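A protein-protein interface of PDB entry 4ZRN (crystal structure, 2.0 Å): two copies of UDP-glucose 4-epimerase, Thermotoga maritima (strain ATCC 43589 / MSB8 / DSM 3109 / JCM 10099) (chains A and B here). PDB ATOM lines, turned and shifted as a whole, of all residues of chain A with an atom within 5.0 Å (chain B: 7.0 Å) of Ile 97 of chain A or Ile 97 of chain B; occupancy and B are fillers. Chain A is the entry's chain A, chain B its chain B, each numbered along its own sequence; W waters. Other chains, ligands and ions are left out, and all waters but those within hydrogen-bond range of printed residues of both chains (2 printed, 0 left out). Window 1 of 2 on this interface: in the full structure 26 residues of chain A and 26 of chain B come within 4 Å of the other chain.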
ATOM      1  N   ASP A  92      22.593   9.059 -34.252  1.00  0.00           N
ATOM      2  CA  ASP A  92      23.972   9.358 -33.899  1.00  0.00           C
ATOM      3  C   ASP A  92      24.403   8.521 -32.704  1.00  0.00           C
ATOM      4  O   ASP A  92      25.465   7.909 -32.725  1.00  0.00           O
ATOM      5  CB  ASP A  92      24.161  10.859 -33.596  1.00  0.00           C
ATOM      6  CG  ASP A  92      25.559  11.186 -33.095  1.00  0.00           C
ATOM      7  OD1 ASP A  92      26.420  11.561 -33.927  1.00  0.00           O
ATOM      8  OD2 ASP A  92      25.814  11.082 -31.860  1.00  0.00           O
ATOM      9  N   ALA A  93      23.573   8.478 -31.668  1.00  0.00           N
ATOM     10  CA  ALA A  93      23.932   7.737 -30.464  1.00  0.00           C
ATOM     11  C   ALA A  93      23.943   6.223 -30.690  1.00  0.00           C
ATOM     12  O   ALA A  93      24.655   5.505 -30.001  1.00  0.00           O
ATOM     13  CB  ALA A  93      23.021   8.119 -29.289  1.00  0.00           C
ATOM     14  N   LYS A  94      23.160   5.733 -31.648  1.00  0.00           N
ATOM     15  CA  LYS A  94      23.202   4.308 -31.986  1.00  0.00           C
ATOM     16  C   LYS A  94      24.594   3.909 -32.469  1.00  0.00           C
ATOM     17  O   LYS A  94      25.120   2.870 -32.093  1.00  0.00           O
ATOM     18  CB  LYS A  94      22.162   3.966 -33.059  1.00  0.00           C
ATOM     19  CG  LYS A  94      20.752   3.735 -32.501  1.00  0.00           C
ATOM     20  CD  LYS A  94      19.723   3.646 -33.632  1.00  0.00           C
ATOM     21  CE  LYS A  94      18.341   3.351 -33.074  1.00  0.00           C
ATOM     22  NZ  LYS A  94      17.233   3.606 -34.057  1.00  0.00           N
ATOM     23  N   THR A  95      25.198   4.738 -33.307  1.00  0.00           N
ATOM     24  CA  THR A  95      26.547   4.440 -33.766  1.00  0.00           C
ATOM     25  C   THR A  95      27.554   4.781 -32.679  1.00  0.00           C
ATOM     26  O   THR A  95      28.421   3.967 -32.336  1.00  0.00           O
ATOM     27  CB  THR A  95      26.899   5.234 -35.034  1.00  0.00           C
ATOM     28  OG1 THR A  95      26.179   4.695 -36.142  1.00  0.00           O
ATOM     29  CG2 THR A  95      28.392   5.127 -35.334  1.00  0.00           C
ATOM     30  N   ASN A  96      27.440   5.991 -32.138  1.00  0.00           N
ATOM     31  CA  ASN A  96      28.473   6.520 -31.249  1.00  0.00           C
ATOM     32  C   ASN A  96      28.511   5.922 -29.850  1.00  0.00           C
ATOM     33  O   ASN A  96      29.587   5.776 -29.272  1.00  0.00           O
ATOM     34  CB  ASN A  96      28.397   8.038 -31.183  1.00  0.00           C
ATOM     35  CG  ASN A  96      28.814   8.680 -32.482  1.00  0.00           C
ATOM     36  OD1 ASN A  96      29.493   8.048 -33.305  1.00  0.00           O
ATOM     37  ND2 ASN A  96      28.411   9.933 -32.686  1.00  0.00           N
ATOM     38  N   ILE A  97      27.355   5.573 -29.302  1.00  0.00           N
ATOM     39  CA  ILE A  97      27.339   4.964 -27.972  1.00  0.00           C
ATOM     40  C   ILE A  97      27.114   3.457 -28.065  1.00  0.00           C
ATOM     41  O   ILE A  97      27.943   2.678 -27.604  1.00  0.00           O
ATOM     42  CB  ILE A  97      26.241   5.571 -27.081  1.00  0.00           C
ATOM     43  CG1 ILE A  97      26.392   7.087 -27.004  1.00  0.00           C
ATOM     44  CG2 ILE A  97      26.304   4.980 -25.682  1.00  0.00           C
ATOM     45  CD1 ILE A  97      25.367   7.774 -26.051  1.00  0.00           C
ATOM     46  N   ILE A  98      25.996   3.054 -28.663  1.00  0.00           N
ATOM     47  CA  ILE A  98      25.634   1.636 -28.742  1.00  0.00           C
ATOM     48  C   ILE A  98      26.680   0.862 -29.535  1.00  0.00           C
ATOM     49  O   ILE A  98      27.099  -0.224 -29.126  1.00  0.00           O
ATOM     50  CB  ILE A  98      24.233   1.416 -29.372  1.00  0.00           C
ATOM     51  CG1 ILE A  98      23.171   2.234 -28.630  1.00  0.00           C
ATOM     52  CG2 ILE A  98      23.866  -0.073 -29.371  1.00  0.00           C
ATOM     53  CD1 ILE A  98      23.226   2.095 -27.104  1.00  0.00           C
ATOM     54  N   GLY A  99      27.112   1.427 -30.664  1.00  0.00           N
ATOM     55  CA  GLY A  99      28.186   0.822 -31.440  1.00  0.00           C
ATOM     56  C   GLY A  99      29.428   0.568 -30.603  1.00  0.00           C
ATOM     57  O   GLY A  99      30.009  -0.526 -30.627  1.00  0.00           O
ATOM     58  N   SER A 100      29.833   1.577 -29.840  1.00  0.00           N
ATOM     59  CA  SER A 100      30.986   1.434 -28.965  1.00  0.00           C
ATOM     60  C   SER A 100      30.806   0.330 -27.927  1.00  0.00           C
ATOM     61  O   SER A 100      31.734  -0.457 -27.668  1.00  0.00           O
ATOM     62  CB  SER A 100      31.272   2.757 -28.266  1.00  0.00           C
ATOM     63  OG  SER A 100      31.644   3.744 -29.211  1.00  0.00           O
ATOM     64  N   LEU A 101      29.627   0.289 -27.315  1.00  0.00           N
ATOM     65  CA  LEU A 101      29.329  -0.705 -26.281  1.00  0.00           C
ATOM     66  C   LEU A 101      29.339  -2.137 -26.832  1.00  0.00           C
ATOM     67  O   LEU A 101      29.784  -3.061 -26.145  1.00  0.00           O
ATOM     68  CB  LEU A 101      27.977  -0.394 -25.606  1.00  0.00           C
ATOM     69  CG  LEU A 101      28.015   0.855 -24.700  1.00  0.00           C
ATOM     70  CD1 LEU A 101      26.635   1.218 -24.159  1.00  0.00           C
ATOM     71  CD2 LEU A 101      28.985   0.627 -23.553  1.00  0.00           C
ATOM     72  N   ALA A 149      27.629  12.061 -26.785  1.00  0.00           N
ATOM     73  CA  ALA A 149      27.882  10.644 -27.104  1.00  0.00           C
ATOM     74  C   ALA A 149      29.343  10.250 -26.897  1.00  0.00           C
ATOM     75  O   ALA A 149      29.630   9.183 -26.328  1.00  0.00           O
ATOM     76  CB  ALA A 149      27.429  10.299 -28.529  1.00  0.00           C
ATOM     77  N   SER A 152      29.906  10.166 -23.119  1.00  0.00           N
ATOM     78  CA  SER A 152      29.263   8.982 -22.532  1.00  0.00           C
ATOM     79  C   SER A 152      30.109   7.742 -22.771  1.00  0.00           C
ATOM     80  O   SER A 152      30.281   6.907 -21.875  1.00  0.00           O
ATOM     81  CB  SER A 152      27.858   8.769 -23.108  1.00  0.00           C
ATOM     82  OG  SER A 152      27.069   9.928 -22.880  1.00  0.00           O
ATOM     83  N   THR A 153      30.658   7.624 -23.974  1.00  0.00           N
ATOM     84  CA  THR A 153      31.493   6.468 -24.299  1.00  0.00           C
ATOM     85  C   THR A 153      32.794   6.468 -23.485  1.00  0.00           C
ATOM     86  O   THR A 153      33.236   5.406 -23.035  1.00  0.00           O
ATOM     87  CB  THR A 153      31.761   6.369 -25.818  1.00  0.00           C
ATOM     88  OG1 THR A 153      30.516   6.119 -26.487  1.00  0.00           O
ATOM     89  CG2 THR A 153      32.722   5.220 -26.130  1.00  0.00           C
ATOM     90  N   TYR A 156      31.946   4.980 -20.204  1.00  0.00           N
ATOM     91  CA  TYR A 156      31.786   3.532 -20.309  1.00  0.00           C
ATOM     92  C   TYR A 156      33.139   2.839 -20.360  1.00  0.00           C
ATOM     93  O   TYR A 156      33.296   1.726 -19.838  1.00  0.00           O
ATOM     94  CB  TYR A 156      30.956   3.156 -21.535  1.00  0.00           C
ATOM     95  CG  TYR A 156      29.453   3.260 -21.347  1.00  0.00           C
ATOM     96  CD1 TYR A 156      28.698   4.181 -22.071  1.00  0.00           C
ATOM     97  CD2 TYR A 156      28.789   2.427 -20.463  1.00  0.00           C
ATOM     98  CE1 TYR A 156      27.327   4.271 -21.914  1.00  0.00           C
ATOM     99  CE2 TYR A 156      27.402   2.501 -20.303  1.00  0.00           C
ATOM    100  CZ  TYR A 156      26.684   3.422 -21.035  1.00  0.00           C
ATOM    101  OH  TYR A 156      25.317   3.502 -20.877  1.00  0.00           O
ATOM    102  N   ILE B  55       9.769   2.194 -25.951  1.00  0.00           N
ATOM    103  CA  ILE B  55      10.086   3.603 -26.156  1.00  0.00           C
ATOM    104  C   ILE B  55      11.120   3.834 -27.257  1.00  0.00           C
ATOM    105  O   ILE B  55      11.132   4.902 -27.869  1.00  0.00           O
ATOM    106  CB  ILE B  55      10.563   4.293 -24.864  1.00  0.00           C
ATOM    107  CG1 ILE B  55      11.795   3.594 -24.284  1.00  0.00           C
ATOM    108  CG2 ILE B  55       9.429   4.374 -23.824  1.00  0.00           C
ATOM    109  CD1 ILE B  55      12.439   4.390 -23.132  1.00  0.00           C
ATOM    110  N   HIS B  75       8.774  10.627 -17.972  1.00  0.00           N
ATOM    111  CA  HIS B  75       9.576   9.539 -18.518  1.00  0.00           C
ATOM    112  C   HIS B  75      10.164   8.682 -17.389  1.00  0.00           C
ATOM    113  O   HIS B  75      11.192   9.030 -16.781  1.00  0.00           O
ATOM    114  CB  HIS B  75      10.653  10.090 -19.461  1.00  0.00           C
ATOM    115  CG  HIS B  75      11.567   9.039 -20.018  1.00  0.00           C
ATOM    116  ND1 HIS B  75      11.156   7.743 -20.259  1.00  0.00           N
ATOM    117  CD2 HIS B  75      12.872   9.094 -20.371  1.00  0.00           C
ATOM    118  CE1 HIS B  75      12.176   7.044 -20.731  1.00  0.00           C
ATOM    119  NE2 HIS B  75      13.228   7.840 -20.809  1.00  0.00           N
ATOM    120  N   ALA B  90      25.083  -2.653 -23.575  1.00  0.00           N
ATOM    121  CA  ALA B  90      24.552  -2.131 -24.829  1.00  0.00           C
ATOM    122  C   ALA B  90      23.034  -2.192 -24.802  1.00  0.00           C
ATOM    123  O   ALA B  90      22.357  -1.248 -25.200  1.00  0.00           O
ATOM    124  CB  ALA B  90      25.120  -2.891 -26.057  1.00  0.00           C
ATOM    125  N   ASP B  92      21.162  -2.291 -22.122  1.00  0.00           N
ATOM    126  CA  ASP B  92      20.740  -1.305 -21.136  1.00  0.00           C
ATOM    127  C   ASP B  92      20.667   0.111 -21.728  1.00  0.00           C
ATOM    128  O   ASP B  92      19.663   0.809 -21.560  1.00  0.00           O
ATOM    129  CB  ASP B  92      21.676  -1.325 -19.926  1.00  0.00           C
ATOM    130  CG  ASP B  92      21.327  -0.269 -18.901  1.00  0.00           C
ATOM    131  OD1 ASP B  92      20.605  -0.607 -17.940  1.00  0.00           O
ATOM    132  OD2 ASP B  92      21.773   0.902 -19.042  1.00  0.00           O
ATOM    133  N   ALA B  93      21.727   0.529 -22.418  1.00  0.00           N
ATOM    134  CA  ALA B  93      21.773   1.865 -23.011  1.00  0.00           C
ATOM    135  C   ALA B  93      20.734   2.045 -24.116  1.00  0.00           C
ATOM    136  O   ALA B  93      20.286   3.168 -24.387  1.00  0.00           O
ATOM    137  CB  ALA B  93      23.179   2.182 -23.523  1.00  0.00           C
ATOM    138  N   LYS B  94      20.346   0.954 -24.768  1.00  0.00           N
ATOM    139  CA  LYS B  94      19.307   1.058 -25.791  1.00  0.00           C
ATOM    140  C   LYS B  94      17.988   1.542 -25.186  1.00  0.00           C
ATOM    141  O   LYS B  94      17.311   2.389 -25.762  1.00  0.00           O
ATOM    142  CB  LYS B  94      19.085  -0.271 -26.518  1.00  0.00           C
ATOM    143  CG  LYS B  94      20.093  -0.570 -27.637  1.00  0.00           C
ATOM    144  CD  LYS B  94      19.508  -1.593 -28.639  1.00  0.00           C
ATOM    145  CE  LYS B  94      19.861  -3.032 -28.283  1.00  0.00           C
ATOM    146  NZ  LYS B  94      21.269  -3.395 -28.658  1.00  0.00           N
ATOM    147  N   THR B  95      17.611   0.994 -24.034  1.00  0.00           N
ATOM    148  CA  THR B  95      16.429   1.496 -23.338  1.00  0.00           C
ATOM    149  C   THR B  95      16.719   2.837 -22.670  1.00  0.00           C
ATOM    150  O   THR B  95      15.951   3.805 -22.822  1.00  0.00           O
ATOM    151  CB  THR B  95      15.903   0.490 -22.284  1.00  0.00           C
ATOM    152  OG1 THR B  95      15.235  -0.585 -22.950  1.00  0.00           O
ATOM    153  CG2 THR B  95      14.894   1.158 -21.360  1.00  0.00           C
ATOM    154  N   ASN B  96      17.842   2.914 -21.961  1.00  0.00           N
ATOM    155  CA  ASN B  96      18.071   4.060 -21.076  1.00  0.00           C
ATOM    156  C   ASN B  96      18.484   5.342 -21.798  1.00  0.00           C
ATOM    157  O   ASN B  96      18.045   6.427 -21.432  1.00  0.00           O
ATOM    158  CB  ASN B  96      19.036   3.691 -19.946  1.00  0.00           C
ATOM    159  CG  ASN B  96      18.390   2.776 -18.933  1.00  0.00           C
ATOM    160  OD1 ASN B  96      17.164   2.748 -18.822  1.00  0.00           O
ATOM    161  ND2 ASN B  96      19.199   2.029 -18.186  1.00  0.00           N
ATOM    162  N   ILE B  97      19.302   5.215 -22.837  1.00  0.00           N
ATOM    163  CA  ILE B  97      19.703   6.392 -23.614  1.00  0.00           C
ATOM    164  C   ILE B  97      18.909   6.527 -24.921  1.00  0.00           C
ATOM    165  O   ILE B  97      18.233   7.540 -25.142  1.00  0.00           O
ATOM    166  CB  ILE B  97      21.236   6.397 -23.903  1.00  0.00           C
ATOM    167  CG1 ILE B  97      22.022   6.262 -22.600  1.00  0.00           C
ATOM    168  CG2 ILE B  97      21.666   7.685 -24.621  1.00  0.00           C
ATOM    169  CD1 ILE B  97      23.548   6.211 -22.796  1.00  0.00           C
ATOM    170  N   ILE B  98      18.990   5.520 -25.793  1.00  0.00           N
ATOM    171  CA  ILE B  98      18.317   5.597 -27.101  1.00  0.00           C
ATOM    172  C   ILE B  98      16.809   5.797 -26.945  1.00  0.00           C
ATOM    173  O   ILE B  98      16.212   6.635 -27.622  1.00  0.00           O
ATOM    174  CB  ILE B  98      18.615   4.360 -27.995  1.00  0.00           C
ATOM    175  CG1 ILE B  98      20.121   4.097 -28.079  1.00  0.00           C
ATOM    176  CG2 ILE B  98      18.012   4.535 -29.400  1.00  0.00           C
ATOM    177  CD1 ILE B  98      20.948   5.267 -28.624  1.00  0.00           C
ATOM    178  N   GLY B  99      16.190   5.038 -26.040  1.00  0.00           N
ATOM    179  CA  GLY B  99      14.774   5.217 -25.750  1.00  0.00           C
ATOM    180  C   GLY B  99      14.417   6.641 -25.357  1.00  0.00           C
ATOM    181  O   GLY B  99      13.419   7.184 -25.843  1.00  0.00           O
ATOM    182  N   SER B 100      15.224   7.248 -24.484  1.00  0.00           N
ATOM    183  CA  SER B 100      14.979   8.627 -24.058  1.00  0.00           C
ATOM    184  C   SER B 100      15.090   9.573 -25.256  1.00  0.00           C
ATOM    185  O   SER B 100      14.294  10.496 -25.411  1.00  0.00           O
ATOM    186  CB  SER B 100      16.011   9.054 -23.017  1.00  0.00           C
ATOM    187  OG  SER B 100      15.947   8.260 -21.847  1.00  0.00           O
ATOM    188  N   LEU B 101      16.099   9.329 -26.088  1.00  0.00           N
ATOM    189  CA  LEU B 101      16.348  10.139 -27.281  1.00  0.00           C
ATOM    190  C   LEU B 101      15.197  10.068 -28.288  1.00  0.00           C
ATOM    191  O   LEU B 101      14.852  11.080 -28.917  1.00  0.00           O
ATOM    192  CB  LEU B 101      17.669   9.729 -27.942  1.00  0.00           C
ATOM    193  CG  LEU B 101      18.926  10.144 -27.166  1.00  0.00           C
ATOM    194  CD1 LEU B 101      20.179   9.707 -27.895  1.00  0.00           C
ATOM    195  CD2 LEU B 101      18.944  11.662 -26.960  1.00  0.00           C
ATOM    196  N   VAL B 102      14.601   8.888 -28.449  1.00  0.00           N
ATOM    197  CA  VAL B 102      13.455   8.770 -29.357  1.00  0.00           C
ATOM    198  C   VAL B 102      12.276   9.598 -28.835  1.00  0.00           C
ATOM    199  O   VAL B 102      11.635  10.341 -29.593  1.00  0.00           O
ATOM    200  CB  VAL B 102      13.037   7.295 -29.577  1.00  0.00           C
ATOM    201  CG1 VAL B 102      11.716   7.205 -30.359  1.00  0.00           C
ATOM    202  CG2 VAL B 102      14.162   6.506 -30.285  1.00  0.00           C
ATOM    203  N   LEU B 103      11.997   9.475 -27.542  1.00  0.00           N
ATOM    204  CA  LEU B 103      10.937  10.259 -26.898  1.00  0.00           C
ATOM    205  C   LEU B 103      11.169  11.757 -27.041  1.00  0.00           C
ATOM    206  O   LEU B 103      10.230  12.525 -27.253  1.00  0.00           O
ATOM    207  CB  LEU B 103      10.832   9.896 -25.412  1.00  0.00           C
ATOM    208  CG  LEU B 103      10.413   8.455 -25.098  1.00  0.00           C
ATOM    209  CD1 LEU B 103      10.638   8.156 -23.624  1.00  0.00           C
ATOM    210  CD2 LEU B 103       8.956   8.231 -25.469  1.00  0.00           C
ATOM    211  N   LEU B 104      12.422  12.176 -26.913  1.00  0.00           N
ATOM    212  CA  LEU B 104      12.755  13.586 -26.985  1.00  0.00           C
ATOM    213  C   LEU B 104      12.620  14.116 -28.409  1.00  0.00           C
ATOM    214  O   LEU B 104      12.131  15.226 -28.614  1.00  0.00           O
ATOM    215  CB  LEU B 104      14.166  13.838 -26.423  1.00  0.00           C
ATOM    216  CG  LEU B 104      14.221  13.756 -24.891  1.00  0.00           C
ATOM    217  CD1 LEU B 104      15.640  13.547 -24.356  1.00  0.00           C
ATOM    218  CD2 LEU B 104      13.582  15.011 -24.288  1.00  0.00           C
ATOM    219  N   PRO B 145      26.998   1.294 -15.503  1.00  0.00           N
ATOM    220  CA  PRO B 145      26.336   1.625 -16.770  1.00  0.00           C
ATOM    221  C   PRO B 145      24.987   2.311 -16.558  1.00  0.00           C
ATOM    222  O   PRO B 145      24.606   3.200 -17.340  1.00  0.00           O
ATOM    223  CB  PRO B 145      26.181   0.253 -17.448  1.00  0.00           C
ATOM    224  CG  PRO B 145      27.381  -0.543 -16.909  1.00  0.00           C
ATOM    225  CD  PRO B 145      27.404  -0.126 -15.447  1.00  0.00           C
ATOM    226  N   ILE B 148      25.819   5.944 -15.670  1.00  0.00           N
ATOM    227  CA  ILE B 148      26.341   6.605 -16.867  1.00  0.00           C
ATOM    228  C   ILE B 148      25.197   6.932 -17.822  1.00  0.00           C
ATOM    229  O   ILE B 148      25.101   8.050 -18.325  1.00  0.00           O
ATOM    230  CB  ILE B 148      27.418   5.736 -17.565  1.00  0.00           C
ATOM    231  CG1 ILE B 148      28.644   5.568 -16.641  1.00  0.00           C
ATOM    232  CG2 ILE B 148      27.844   6.373 -18.909  1.00  0.00           C
ATOM    233  CD1 ILE B 148      29.631   4.460 -17.074  1.00  0.00           C
ATOM    234  N   ALA B 149      24.316   5.962 -18.048  1.00  0.00           N
ATOM    235  CA  ALA B 149      23.172   6.142 -18.950  1.00  0.00           C
ATOM    236  C   ALA B 149      22.232   7.236 -18.456  1.00  0.00           C
ATOM    237  O   ALA B 149      21.758   8.048 -19.246  1.00  0.00           O
ATOM    238  CB  ALA B 149      22.390   4.818 -19.104  1.00  0.00           C
ATOM    239  N   LYS B 150      21.937   7.248 -17.156  1.00  0.00           N
ATOM    240  CA  LYS B 150      21.060   8.288 -16.616  1.00  0.00           C
ATOM    241  C   LYS B 150      21.691   9.677 -16.779  1.00  0.00           C
ATOM    242  O   LYS B 150      21.031  10.641 -17.183  1.00  0.00           O
ATOM    243  CB  LYS B 150      20.760   8.009 -15.138  1.00  0.00           C
ATOM    244  CG  LYS B 150      19.724   6.900 -14.901  1.00  0.00           C
ATOM    245  CD  LYS B 150      18.358   7.269 -15.499  1.00  0.00           C
ATOM    246  CE  LYS B 150      17.277   6.278 -15.034  1.00  0.00           C
ATOM    247  NZ  LYS B 150      15.979   6.563 -15.688  1.00  0.00           N
ATOM    248  N   SER B 152      24.029  10.556 -18.991  1.00  0.00           N
ATOM    249  CA  SER B 152      24.030  10.901 -20.415  1.00  0.00           C
ATOM    250  C   SER B 152      22.687  11.486 -20.824  1.00  0.00           C
ATOM    251  O   SER B 152      22.626  12.479 -21.544  1.00  0.00           O
ATOM    252  CB  SER B 152      24.342   9.685 -21.301  1.00  0.00           C
ATOM    253  OG  SER B 152      25.562   9.098 -20.895  1.00  0.00           O
ATOM    254  N   THR B 153      21.606  10.857 -20.381  1.00  0.00           N
ATOM    255  CA  THR B 153      20.284  11.381 -20.704  1.00  0.00           C
ATOM    256  C   THR B 153      20.067  12.785 -20.143  1.00  0.00           C
ATOM    257  O   THR B 153      19.466  13.628 -20.815  1.00  0.00           O
ATOM    258  CB  THR B 153      19.155  10.409 -20.263  1.00  0.00           C
ATOM    259  OG1 THR B 153      19.293   9.184 -21.000  1.00  0.00           O
ATOM    260  CG2 THR B 153      17.786  11.012 -20.561  1.00  0.00           C
ATOM    261  N   TYR B 156      21.655  15.076 -22.521  1.00  0.00           N
ATOM    262  CA  TYR B 156      20.871  15.226 -23.743  1.00  0.00           C
ATOM    263  C   TYR B 156      19.669  16.150 -23.510  1.00  0.00           C
ATOM    264  O   TYR B 156      19.277  16.937 -24.388  1.00  0.00           O
ATOM    265  CB  TYR B 156      20.410  13.852 -24.246  1.00  0.00           C
ATOM    266  CG  TYR B 156      21.427  13.092 -25.073  1.00  0.00           C
ATOM    267  CD1 TYR B 156      21.951  11.884 -24.628  1.00  0.00           C
ATOM    268  CD2 TYR B 156      21.828  13.560 -26.318  1.00  0.00           C
ATOM    269  CE1 TYR B 156      22.861  11.168 -25.391  1.00  0.00           C
ATOM    270  CE2 TYR B 156      22.741  12.846 -27.096  1.00  0.00           C
ATOM    271  CZ  TYR B 156      23.249  11.650 -26.618  1.00  0.00           C
ATOM    272  OH  TYR B 156      24.148  10.928 -27.372  1.00  0.00           O
HETATM  273  O   HOH W   1      24.268   1.216 -20.097  1.00  0.00           O
HETATM  274  O   HOH W   2      23.855  11.456 -29.987  1.00  0.00           O
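OG of Ser 152 of chain A sits at hydrogen-bond distance from OG of Ser 152 of chain B (2.6 Å).
The backbone carbonyl oxygen of Ala 93 of chain A sits at hydrogen-bond distance from the backbone NH of Ile 98 of chain A (3.1 Å).
The backbone carbonyl oxygen (O) of Lys 94 of chain A sits at hydrogen-bond distance from the backbone NH (N) of Gly 99 of chain A (2.8 Å).
The backbone carbonyl oxygen of Ala 149 of chain B is in hydrogen-bond range of the side-chain hydroxyl of Thr 153 of chain B, at 3.2 Å.
The backbone NH (N) of Ile 98 of chain B sits at hydrogen-bond distance from the backbone carbonyl oxygen (O) of Ala 93 of chain B.
The backbone carbonyl oxygen (O) of Ala 149 of chain A lies within hydrogen-bond range of the side-chain hydroxyl (OG1) of Thr 153 of chain A (3.2 Å).
O of Ile 148 of chain B sits at hydrogen-bond distance from OG of Ser 152 of chain B (2.8 Å).
Among the printed residues, merely in contact across the chains: Ala 149 of chain A with Tyr 156 of chain B (3.5 Å), Ala 93 of chain A with Leu 101 of chain B (3.5 Å), Ile 98 of chain A with Ala 93 of chain B (3.6 Å), Ala 93 of chain A with Tyr 156 of chain B (3.6 Å), Ala 93 of chain A with Ile 98 of chain B (3.6 Å), Ile 98 of chain A with Ile 98 of chain B (3.6 Å), Tyr 156 of chain A with Pro 145 of chain B (3.6 Å), Ile 97 of chain A with Tyr 156 of chain B (3.6 Å), Leu 101 of chain A with Ala 93 of chain B (3.6 Å), Tyr 156 of chain A with Ala 93 of chain B (3.6 Å), Tyr 156 of chain A with Ala 149 of chain B (3.7 Å), Tyr 156 of chain A with Ile 148 of chain B (3.7 Å), Tyr 156 of chain A with Ile 97 of chain B (3.8 Å), Lys 94 of chain A with Ile 98 of chain B (3.8 Å), Leu 101 of chain A with Ala 90 of chain B (3.8 Å), Ser 152 of chain A with Ile 148 of chain B (3.9 Å), Ile 98 of chain A with Lys 94 of chain B (3.9 Å), Ile 98 of chain A with Ala 90 of chain B (3.9 Å) and Ile 97 of chain A with Ile 97 of chain B (3.97 Å).
Of chain B, only Ile 97 (3.97 Å) and Tyr 156 (3.6 Å) come within 4 Å of Ile 97 of chain A.
Of chain A, only Ile 97 and Tyr 156 come within 4 Å of Ile 97 of chain B.
Printed residues of chain A within 4 Å of Ile 98 of chain B: Ala 93, Lys 94 and Ile 98.
Printed residues of chain A within 4 Å of Pro 145 of chain B: Tyr 156.
Printed residues of chain B within 4 Å of Leu 101 of chain A: Ala 90 (3.8 Å) and Ala 93 (3.6 Å).
Asn 96 of chain B touches none of the printed residues of chain A.
Asp 92 of chain B touches none of the printed residues of chain A.
The nearest residue of chain A that does not touch Ile 97 of chain B is Ala 93 of chain A (4.9 Å).
Hydrophobic or aromatic side chains of chain B that line the printed part of chain A: Ala 90, Ala 93, Ile 97, Ile 98, Leu 101, Pro 145, Ile 148, Ala 149 and Tyr 156.
Hydrophobic or aromatic side chains of chain A that line the printed part of chain B: Ala 93, Ile 97, Ile 98, Leu 101, Ala 149 and Tyr 156.
Among the printed residues, 20 pairs touch across the chains.
Among the printed residues, no Asp or Glu carboxylate lies within 4 Å of a Lys or Arg side-chain nitrogen of the other chain.
Ala 93 of chain A touches Leu 101 of chain B, and with the chains exchanged Leu 101 of chain A touches Ala 93 of chain B.
Ala 93 of chain A touches Tyr 156 of chain B, and with the chains exchanged Tyr 156 of chain A touches Ala 93 of chain B.
Ile 97 of chain A touches Tyr 156 of chain B, and with the chains exchanged Tyr 156 of chain A touches Ile 97 of chain B.
Ile 98 of chain B touches its own counterpart, Ile 98 of chain A.
Of the 20 pairs that touch across the chains among the printed residues, 15 have their exchanged pair printed and touching as well.
Water W1 lies within hydrogen-bond range of OH of Tyr 156 of chain A (2.6 Å), OD2 of Asp 92 of chain B (2.7 Å) and O of Pro 145 of chain B (3.4 Å).
Water W2 lies within hydrogen-bond range of OH of Tyr 156 of chain B, OD2 of Asp 92 of chain A and N of Ala 93 of chain A.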
